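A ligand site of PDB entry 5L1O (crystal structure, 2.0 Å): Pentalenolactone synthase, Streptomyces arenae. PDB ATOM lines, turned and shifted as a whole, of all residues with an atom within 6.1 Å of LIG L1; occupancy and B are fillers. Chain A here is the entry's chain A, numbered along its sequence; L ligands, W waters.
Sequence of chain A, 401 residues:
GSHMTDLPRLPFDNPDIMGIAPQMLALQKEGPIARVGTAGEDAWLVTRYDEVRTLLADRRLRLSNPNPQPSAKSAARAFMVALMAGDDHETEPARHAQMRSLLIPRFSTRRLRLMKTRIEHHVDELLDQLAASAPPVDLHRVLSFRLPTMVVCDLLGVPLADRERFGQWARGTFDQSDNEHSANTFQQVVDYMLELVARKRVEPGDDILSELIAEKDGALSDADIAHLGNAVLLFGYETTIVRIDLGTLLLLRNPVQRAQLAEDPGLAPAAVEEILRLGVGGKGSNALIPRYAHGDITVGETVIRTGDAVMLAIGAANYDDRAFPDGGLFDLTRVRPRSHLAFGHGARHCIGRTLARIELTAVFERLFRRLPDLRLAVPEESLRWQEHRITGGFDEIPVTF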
ATOM      1  N   ARG A  77      14.085 -26.706 -16.604  1.00  0.00           N
ATOM      2  CA  ARG A  77      15.303 -27.115 -17.303  1.00  0.00           C
ATOM      3  C   ARG A  77      15.247 -28.586 -17.693  1.00  0.00           C
ATOM      4  O   ARG A  77      15.777 -28.967 -18.743  1.00  0.00           O
ATOM      5  CB  ARG A  77      16.536 -26.844 -16.438  1.00  0.00           C
ATOM      6  CG  ARG A  77      17.100 -25.448 -16.550  1.00  0.00           C
ATOM      7  CD  ARG A  77      17.798 -25.223 -17.902  1.00  0.00           C
ATOM      8  NE  ARG A  77      18.312 -23.858 -18.005  1.00  0.00           N
ATOM      9  CZ  ARG A  77      18.860 -23.324 -19.091  1.00  0.00           C
ATOM     10  NH1 ARG A  77      18.960 -24.035 -20.216  1.00  0.00           N
ATOM     11  NH2 ARG A  77      19.288 -22.070 -19.062  1.00  0.00           N
ATOM     12  N   MET A  80      13.151 -28.857 -20.858  1.00  0.00           N
ATOM     13  CA  MET A  80      13.915 -28.364 -21.998  1.00  0.00           C
ATOM     14  C   MET A  80      14.913 -29.414 -22.481  1.00  0.00           C
ATOM     15  O   MET A  80      15.005 -29.703 -23.672  1.00  0.00           O
ATOM     16  CB  MET A  80      14.646 -27.069 -21.618  1.00  0.00           C
ATOM     17  CG  MET A  80      15.429 -26.438 -22.779  1.00  0.00           C
ATOM     18  SD  MET A  80      15.911 -24.730 -22.456  1.00  0.00           S
ATOM     19  CE  MET A  80      14.344 -23.877 -22.786  1.00  0.00           C
ATOM     20  N   MET A  84      14.971 -31.890 -26.046  1.00  0.00           N
ATOM     21  CA  MET A  84      16.163 -31.872 -26.895  1.00  0.00           C
ATOM     22  C   MET A  84      16.870 -33.217 -26.915  1.00  0.00           C
ATOM     23  O   MET A  84      18.010 -33.291 -27.394  1.00  0.00           O
ATOM     24  CB  MET A  84      17.113 -30.759 -26.443  1.00  0.00           C
ATOM     25  CG  MET A  84      16.541 -29.348 -26.747  1.00  0.00           C
ATOM     26  SD  MET A  84      17.432 -27.988 -25.943  1.00  0.00           S
ATOM     27  CE  MET A  84      18.907 -27.904 -26.960  1.00  0.00           C
ATOM     28  N   PHE A 174       8.787 -23.076 -19.014  1.00  0.00           N
ATOM     29  CA  PHE A 174      10.171 -22.731 -18.735  1.00  0.00           C
ATOM     30  C   PHE A 174      10.312 -21.756 -17.559  1.00  0.00           C
ATOM     31  O   PHE A 174      11.299 -21.029 -17.460  1.00  0.00           O
ATOM     32  CB  PHE A 174      10.849 -22.191 -19.993  1.00  0.00           C
ATOM     33  CG  PHE A 174      10.854 -23.197 -21.130  1.00  0.00           C
ATOM     34  CD1 PHE A 174      11.034 -24.543 -20.869  1.00  0.00           C
ATOM     35  CD2 PHE A 174      10.653 -22.791 -22.451  1.00  0.00           C
ATOM     36  CE1 PHE A 174      11.024 -25.488 -21.891  1.00  0.00           C
ATOM     37  CE2 PHE A 174      10.638 -23.733 -23.482  1.00  0.00           C
ATOM     38  CZ  PHE A 174      10.814 -25.082 -23.198  1.00  0.00           C
ATOM     39  N   LEU A 234       7.171 -25.296 -28.392  1.00  0.00           N
ATOM     40  CA  LEU A 234       7.796 -24.636 -27.235  1.00  0.00           C
ATOM     41  C   LEU A 234       9.074 -23.891 -27.608  1.00  0.00           C
ATOM     42  O   LEU A 234       9.418 -22.921 -26.934  1.00  0.00           O
ATOM     43  CB  LEU A 234       8.075 -25.669 -26.138  1.00  0.00           C
ATOM     44  CG  LEU A 234       6.818 -26.190 -25.435  1.00  0.00           C
ATOM     45  CD1 LEU A 234       7.101 -27.372 -24.544  1.00  0.00           C
ATOM     46  CD2 LEU A 234       6.160 -25.086 -24.612  1.00  0.00           C
ATOM     47  N   PHE A 235       9.791 -24.307 -28.662  1.00  0.00           N
ATOM     48  CA  PHE A 235      10.961 -23.543 -29.108  1.00  0.00           C
ATOM     49  C   PHE A 235      10.670 -22.616 -30.290  1.00  0.00           C
ATOM     50  O   PHE A 235      11.476 -21.734 -30.595  1.00  0.00           O
ATOM     51  CB  PHE A 235      12.127 -24.474 -29.510  1.00  0.00           C
ATOM     52  CG  PHE A 235      12.564 -25.434 -28.407  1.00  0.00           C
ATOM     53  CD1 PHE A 235      13.131 -26.663 -28.738  1.00  0.00           C
ATOM     54  CD2 PHE A 235      12.406 -25.106 -27.065  1.00  0.00           C
ATOM     55  CE1 PHE A 235      13.544 -27.557 -27.738  1.00  0.00           C
ATOM     56  CE2 PHE A 235      12.816 -25.988 -26.045  1.00  0.00           C
ATOM     57  CZ  PHE A 235      13.379 -27.214 -26.385  1.00  0.00           C
ATOM     58  N   THR A 239      11.231 -17.379 -28.423  1.00  0.00           N
ATOM     59  CA  THR A 239      12.511 -16.693 -28.600  1.00  0.00           C
ATOM     60  C   THR A 239      12.453 -15.688 -29.746  1.00  0.00           C
ATOM     61  O   THR A 239      13.124 -14.651 -29.693  1.00  0.00           O
ATOM     62  CB  THR A 239      13.667 -17.693 -28.839  1.00  0.00           C
ATOM     63  OG1 THR A 239      13.404 -18.498 -29.995  1.00  0.00           O
ATOM     64  CG2 THR A 239      13.901 -18.590 -27.608  1.00  0.00           C
ATOM     65  N   ARG A 243      13.221 -11.571 -29.750  1.00  0.00           N
ATOM     66  CA  ARG A 243      14.117 -10.878 -30.679  1.00  0.00           C
ATOM     67  C   ARG A 243      13.438  -9.714 -31.402  1.00  0.00           C
ATOM     68  O   ARG A 243      14.101  -8.731 -31.754  1.00  0.00           O
ATOM     69  CB  ARG A 243      14.718 -11.855 -31.705  1.00  0.00           C
ATOM     70  CG  ARG A 243      15.598 -12.971 -31.085  1.00  0.00           C
ATOM     71  CD  ARG A 243      16.393 -12.414 -29.918  1.00  0.00           C
ATOM     72  NE  ARG A 243      17.308 -13.361 -29.255  1.00  0.00           N
ATOM     73  CZ  ARG A 243      16.939 -14.240 -28.334  1.00  0.00           C
ATOM     74  NH1 ARG A 243      15.661 -14.356 -28.003  1.00  0.00           N
ATOM     75  NH2 ARG A 243      17.843 -15.016 -27.748  1.00  0.00           N
ATOM     76  N   SER A 285      20.935 -14.492 -18.901  1.00  0.00           N
ATOM     77  CA  SER A 285      21.119 -15.902 -18.576  1.00  0.00           C
ATOM     78  C   SER A 285      20.698 -16.833 -19.715  1.00  0.00           C
ATOM     79  O   SER A 285      21.124 -17.990 -19.743  1.00  0.00           O
ATOM     80  CB  SER A 285      20.354 -16.275 -17.303  1.00  0.00           C
ATOM     81  OG  SER A 285      20.797 -15.502 -16.182  1.00  0.00           O
ATOM     82  N   ASN A 286      19.860 -16.348 -20.639  1.00  0.00           N
ATOM     83  CA  ASN A 286      19.483 -17.142 -21.798  1.00  0.00           C
ATOM     84  C   ASN A 286      20.548 -17.109 -22.890  1.00  0.00           C
ATOM     85  O   ASN A 286      20.484 -17.936 -23.815  1.00  0.00           O
ATOM     86  CB  ASN A 286      18.149 -16.653 -22.384  1.00  0.00           C
ATOM     87  CG  ASN A 286      18.218 -15.222 -22.871  1.00  0.00           C
ATOM     88  OD1 ASN A 286      18.643 -14.328 -22.137  1.00  0.00           O
ATOM     89  ND2 ASN A 286      17.774 -14.993 -24.101  1.00  0.00           N
ATOM     90  N   ALA A 287      21.508 -16.188 -22.814  1.00  0.00           N
ATOM     91  CA  ALA A 287      22.601 -16.126 -23.789  1.00  0.00           C
ATOM     92  C   ALA A 287      23.803 -16.978 -23.378  1.00  0.00           C
ATOM     93  O   ALA A 287      24.952 -16.627 -23.694  1.00  0.00           O
ATOM     94  CB  ALA A 287      23.035 -14.673 -24.030  1.00  0.00           C
ATOM     95  N   LEU A 288      23.546 -18.068 -22.665  1.00  0.00           N
ATOM     96  CA  LEU A 288      24.531 -19.091 -22.312  1.00  0.00           C
ATOM     97  C   LEU A 288      24.030 -20.421 -22.843  1.00  0.00           C
ATOM     98  O   LEU A 288      22.862 -20.771 -22.623  1.00  0.00           O
ATOM     99  CB  LEU A 288      24.724 -19.189 -20.798  1.00  0.00           C
ATOM    100  CG  LEU A 288      25.032 -17.897 -20.033  1.00  0.00           C
ATOM    101  CD1 LEU A 288      24.987 -18.176 -18.537  1.00  0.00           C
ATOM    102  CD2 LEU A 288      26.391 -17.373 -20.440  1.00  0.00           C
ATOM    103  N   ILE A 289      24.885 -21.178 -23.515  1.00  0.00           N
ATOM    104  CA  ILE A 289      24.556 -22.531 -23.957  1.00  0.00           C
ATOM    105  C   ILE A 289      25.187 -23.513 -22.973  1.00  0.00           C
ATOM    106  O   ILE A 289      26.422 -23.534 -22.838  1.00  0.00           O
ATOM    107  CB  ILE A 289      25.032 -22.804 -25.383  1.00  0.00           C
ATOM    108  CG1 ILE A 289      24.246 -21.939 -26.383  1.00  0.00           C
ATOM    109  CG2 ILE A 289      24.863 -24.296 -25.685  1.00  0.00           C
ATOM    110  CD1 ILE A 289      24.597 -22.199 -27.865  1.00  0.00           C
ATOM    111  N   PRO A 290      24.407 -24.330 -22.265  1.00  0.00           N
ATOM    112  CA  PRO A 290      24.975 -25.217 -21.236  1.00  0.00           C
ATOM    113  C   PRO A 290      25.435 -26.544 -21.819  1.00  0.00           C
ATOM    114  O   PRO A 290      24.811 -27.107 -22.725  1.00  0.00           O
ATOM    115  CB  PRO A 290      23.795 -25.414 -20.279  1.00  0.00           C
ATOM    116  CG  PRO A 290      22.584 -25.386 -21.194  1.00  0.00           C
ATOM    117  CD  PRO A 290      22.935 -24.449 -22.341  1.00  0.00           C
ATOM    118  N   ILE A 314      27.447 -17.315 -25.557  1.00  0.00           N
ATOM    119  CA  ILE A 314      27.262 -16.833 -26.925  1.00  0.00           C
ATOM    120  C   ILE A 314      26.983 -15.329 -26.946  1.00  0.00           C
ATOM    121  O   ILE A 314      27.426 -14.630 -27.869  1.00  0.00           O
ATOM    122  CB  ILE A 314      26.142 -17.614 -27.644  1.00  0.00           C
ATOM    123  CG1 ILE A 314      24.816 -17.572 -26.874  1.00  0.00           C
ATOM    124  CG2 ILE A 314      26.563 -19.067 -27.898  1.00  0.00           C
ATOM    125  CD1 ILE A 314      23.653 -18.309 -27.555  1.00  0.00           C
ATOM    126  N   ALA A 342      24.389 -16.422 -32.188  1.00  0.00           N
ATOM    127  CA  ALA A 342      23.097 -16.364 -31.496  1.00  0.00           C
ATOM    128  C   ALA A 342      22.193 -17.559 -31.782  1.00  0.00           C
ATOM    129  O   ALA A 342      21.249 -17.815 -31.013  1.00  0.00           O
ATOM    130  CB  ALA A 342      22.344 -15.082 -31.857  1.00  0.00           C
ATOM    131  N   ILE A 390      13.459 -19.282 -18.473  1.00  0.00           N
ATOM    132  CA  ILE A 390      14.682 -19.682 -19.183  1.00  0.00           C
ATOM    133  C   ILE A 390      14.910 -18.774 -20.380  1.00  0.00           C
ATOM    134  O   ILE A 390      16.049 -18.378 -20.674  1.00  0.00           O
ATOM    135  CB  ILE A 390      14.630 -21.153 -19.610  1.00  0.00           C
ATOM    136  CG1 ILE A 390      14.561 -22.079 -18.385  1.00  0.00           C
ATOM    137  CG2 ILE A 390      15.854 -21.501 -20.462  1.00  0.00           C
ATOM    138  CD1 ILE A 390      14.324 -23.539 -18.749  1.00  0.00           C
ATOM    139  N   THR A 391      13.822 -18.408 -21.068  1.00  0.00           N
ATOM    140  CA  THR A 391      13.875 -17.578 -22.255  1.00  0.00           C
ATOM    141  C   THR A 391      13.763 -16.075 -21.965  1.00  0.00           C
ATOM    142  O   THR A 391      13.695 -15.287 -22.917  1.00  0.00           O
ATOM    143  CB  THR A 391      12.755 -17.988 -23.218  1.00  0.00           C
ATOM    144  OG1 THR A 391      11.556 -18.218 -22.465  1.00  0.00           O
ATOM    145  CG2 THR A 391      13.116 -19.287 -23.920  1.00  0.00           C
ATOM    146  N   GLY A 392      13.757 -15.669 -20.692  1.00  0.00           N
ATOM    147  CA  GLY A 392      13.772 -14.240 -20.348  1.00  0.00           C
ATOM    148  C   GLY A 392      12.606 -13.488 -20.957  1.00  0.00           C
ATOM    149  O   GLY A 392      11.445 -13.918 -20.890  1.00  0.00           O
HETATM  150  C1  LIG L   1      17.245 -22.264 -27.885  1.00  0.00           C
HETATM  151  C2  LIG L   1      16.415 -23.109 -26.909  1.00  0.00           C
HETATM  152  C3  LIG L   1      16.180 -24.505 -27.493  1.00  0.00           C
HETATM  153  C4  LIG L   1      15.023 -22.507 -26.626  1.00  0.00           C
HETATM  154  C5  LIG L   1      17.934 -19.942 -27.058  1.00  0.00           C
HETATM  155  C6  LIG L   1      17.759 -20.258 -23.623  1.00  0.00           C
HETATM  156  C7  LIG L   1      20.625 -21.153 -25.197  1.00  0.00           C
HETATM  157  C8  LIG L   1      17.353 -23.175 -25.678  1.00  0.00           C
HETATM  158  C9  LIG L   1      16.930 -18.258 -25.640  1.00  0.00           C
HETATM  159  C10 LIG L   1      19.159 -22.216 -23.457  1.00  0.00           C
HETATM  160  C11 LIG L   1      17.305 -19.543 -25.909  1.00  0.00           C
HETATM  161  C12 LIG L   1      18.238 -21.357 -27.057  1.00  0.00           C
HETATM  162  C13 LIG L   1      17.163 -20.650 -25.020  1.00  0.00           C
HETATM  163  C14 LIG L   1      19.382 -21.935 -24.820  1.00  0.00           C
HETATM  164  C15 LIG L   1      18.045 -21.773 -25.599  1.00  0.00           C
HETATM  165  O1  LIG L   1      17.222 -17.320 -26.408  1.00  0.00           O
HETATM  166  O2  LIG L   1      19.754 -23.133 -22.886  1.00  0.00           O
HETATM  167  O3  LIG L   1      16.242 -17.941 -24.628  1.00  0.00           O
HETATM  168  O4  LIG L   1      18.234 -21.418 -22.842  1.00  0.00           O
HETATM  169  O5  LIG L   1      20.483 -22.584 -25.474  1.00  0.00           O
HETATM  170  C1  LG2 L   2      18.231 -24.761 -31.004  1.00  0.00           C
HETATM  171  C2  LG2 L   2      18.335 -19.901 -30.813  1.00  0.00           C
HETATM  172  C3  LG2 L   2      14.117 -19.751 -33.247  1.00  0.00           C
HETATM  173  C4  LG2 L   2      13.856 -24.587 -33.193  1.00  0.00           C
HETATM  174  C5  LG2 L   2      18.671 -23.467 -30.788  1.00  0.00           C
HETATM  175  C6  LG2 L   2      19.934 -23.072 -30.176  1.00  0.00           C
HETATM  176  C7  LG2 L   2      19.945 -21.734 -30.138  1.00  0.00           C
HETATM  177  C8  LG2 L   2      18.706 -21.237 -30.704  1.00  0.00           C
HETATM  178  C9  LG2 L   2      21.073 -20.833 -29.560  1.00  0.00           C
HETATM  179  C10 LG2 L   2      21.064 -24.040 -29.700  1.00  0.00           C
HETATM  180  C11 LG2 L   2      20.823 -24.606 -28.284  1.00  0.00           C
HETATM  181  C12 LG2 L   2      22.003 -25.473 -27.846  1.00  0.00           C
HETATM  182  O1  LG2 L   2      23.015 -25.591 -28.579  1.00  0.00           O
HETATM  183  O2  LG2 L   2      21.938 -26.071 -26.732  1.00  0.00           O
HETATM  184  C13 LG2 L   2      17.198 -19.413 -31.428  1.00  0.00           C
HETATM  185  C14 LG2 L   2      16.835 -18.020 -31.622  1.00  0.00           C
HETATM  186  C15 LG2 L   2      15.666 -17.997 -32.276  1.00  0.00           C
HETATM  187  C16 LG2 L   2      15.260 -19.370 -32.564  1.00  0.00           C
HETATM  188  C17 LG2 L   2      17.662 -16.819 -31.102  1.00  0.00           C
HETATM  189  C18 LG2 L   2      14.837 -16.783 -32.749  1.00  0.00           C
HETATM  190  C19 LG2 L   2      15.391 -15.633 -33.147  1.00  0.00           C
HETATM  191  C20 LG2 L   2      13.679 -21.037 -33.495  1.00  0.00           C
HETATM  192  C21 LG2 L   2      12.534 -21.411 -34.291  1.00  0.00           C
HETATM  193  C22 LG2 L   2      12.460 -22.765 -34.273  1.00  0.00           C
HETATM  194  C23 LG2 L   2      13.569 -23.267 -33.475  1.00  0.00           C
HETATM  195  C24 LG2 L   2      11.615 -20.375 -34.996  1.00  0.00           C
HETATM  196  C25 LG2 L   2      11.430 -23.716 -34.939  1.00  0.00           C
HETATM  197  C26 LG2 L   2      10.263 -23.305 -35.455  1.00  0.00           C
HETATM  198  C27 LG2 L   2      14.993 -25.045 -32.543  1.00  0.00           C
HETATM  199  C28 LG2 L   2      15.265 -26.415 -32.193  1.00  0.00           C
HETATM  200  C29 LG2 L   2      16.458 -26.477 -31.601  1.00  0.00           C
HETATM  201  C30 LG2 L   2      17.001 -25.127 -31.536  1.00  0.00           C
HETATM  202  C31 LG2 L   2      14.320 -27.603 -32.481  1.00  0.00           C
HETATM  203  C32 LG2 L   2      17.152 -27.736 -31.041  1.00  0.00           C
HETATM  204  C33 LG2 L   2      18.330 -28.123 -31.948  1.00  0.00           C
HETATM  205  C34 LG2 L   2      19.060 -29.328 -31.404  1.00  0.00           C
HETATM  206  O3  LG2 L   2      19.643 -30.092 -32.216  1.00  0.00           O
HETATM  207  O4  LG2 L   2      19.054 -29.551 -30.148  1.00  0.00           O
HETATM  208  N1  LG2 L   2      17.955 -22.328 -31.096  1.00  0.00           N
HETATM  209  N2  LG2 L   2      16.220 -20.193 -32.022  1.00  0.00           N
HETATM  210  N3  LG2 L   2      14.289 -22.183 -33.015  1.00  0.00           N
HETATM  211  N4  LG2 L   2      16.072 -24.288 -32.120  1.00  0.00           N
HETATM  212 FE1  LG2 L   2      16.269 -22.254 -32.307  1.00  0.00          FE
HETATM  213  O   HOH W   1      14.741 -15.596 -25.583  1.00  0.00           O
HETATM  214  O   HOH W   2      20.078 -17.585 -26.580  1.00  0.00           O
HETATM  215  O   HOH W   3      20.560 -25.559 -24.478  1.00  0.00           O
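An oxygen (O1) of LIG L1 sits at hydrogen-bond distance from the side-chain amide nitrogen (ND2) of Asn 286, 3.3 Å away.
The guanidinium group of Arg 77 lies within hydrogen-bond range of an oxygen (O2) of LIG L1.
The guanidinium group (NH2) of Arg 243 lies within salt-bridge range of an oxygen (O1) of LIG L1, at 2.7 Å.
The backbone NH of Ile 390 lies within hydrogen-bond range of the backbone carbonyl oxygen of Phe 174.
The backbone carbonyl oxygen (O) of Thr 239 is in hydrogen-bond range of the guanidinium group (NH1) of Arg 243, at 3.1 Å.
Met 80 touches LIG L1.
CD2 of Phe 235 touches C4 of LIG L1, at 3.7 Å.
Thr 239 touches LIG L1.
Leu 288 touches LIG L1 (O to C7, 3.4 Å).
Ile 289 touches LIG L1.
Pro 290 touches LIG L1 (CD to O2, 3.5 Å).
Ile 390 touches LIG L1.
Thr 391 touches LIG L1.
Hydrophobic or aromatic side chains that line LIG L1: Met 80, Phe 235, Ile 289, Pro 290 and Ile 390.
Within 4 Å of LIG L1: Arg 77, Met 80, Phe 235, Thr 239, Arg 243, Asn 286, Leu 288, Ile 289, Pro 290, Ile 390 and Thr 391.
Along chain A the residues within 4 Å of LIG L1 span positions 77 to 391.
The nearest printed residue that does not touch LIG L1 is Met 84 (4.01 Å).
Water W2 bridges the backbone carbonyl oxygen of Asn 286 (2.8 Å) and an oxygen (O1) of LIG L1 (2.9 Å).
Water W1 lies within hydrogen-bond range of the guanidinium group (NH1) of Arg 243 (2.9 Å), the backbone carbonyl oxygen (O) of Thr 391 (2.9 Å), an oxygen (O3) of LIG L1 (2.9 Å) and the side-chain amide nitrogen (ND2) of Asn 286 (3.4 Å).
Water W3 lies within hydrogen-bond range of an oxygen (O2) of LG2 L2 (2.7 Å) and an oxygen (O2) of LIG L1 (3.0 Å).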
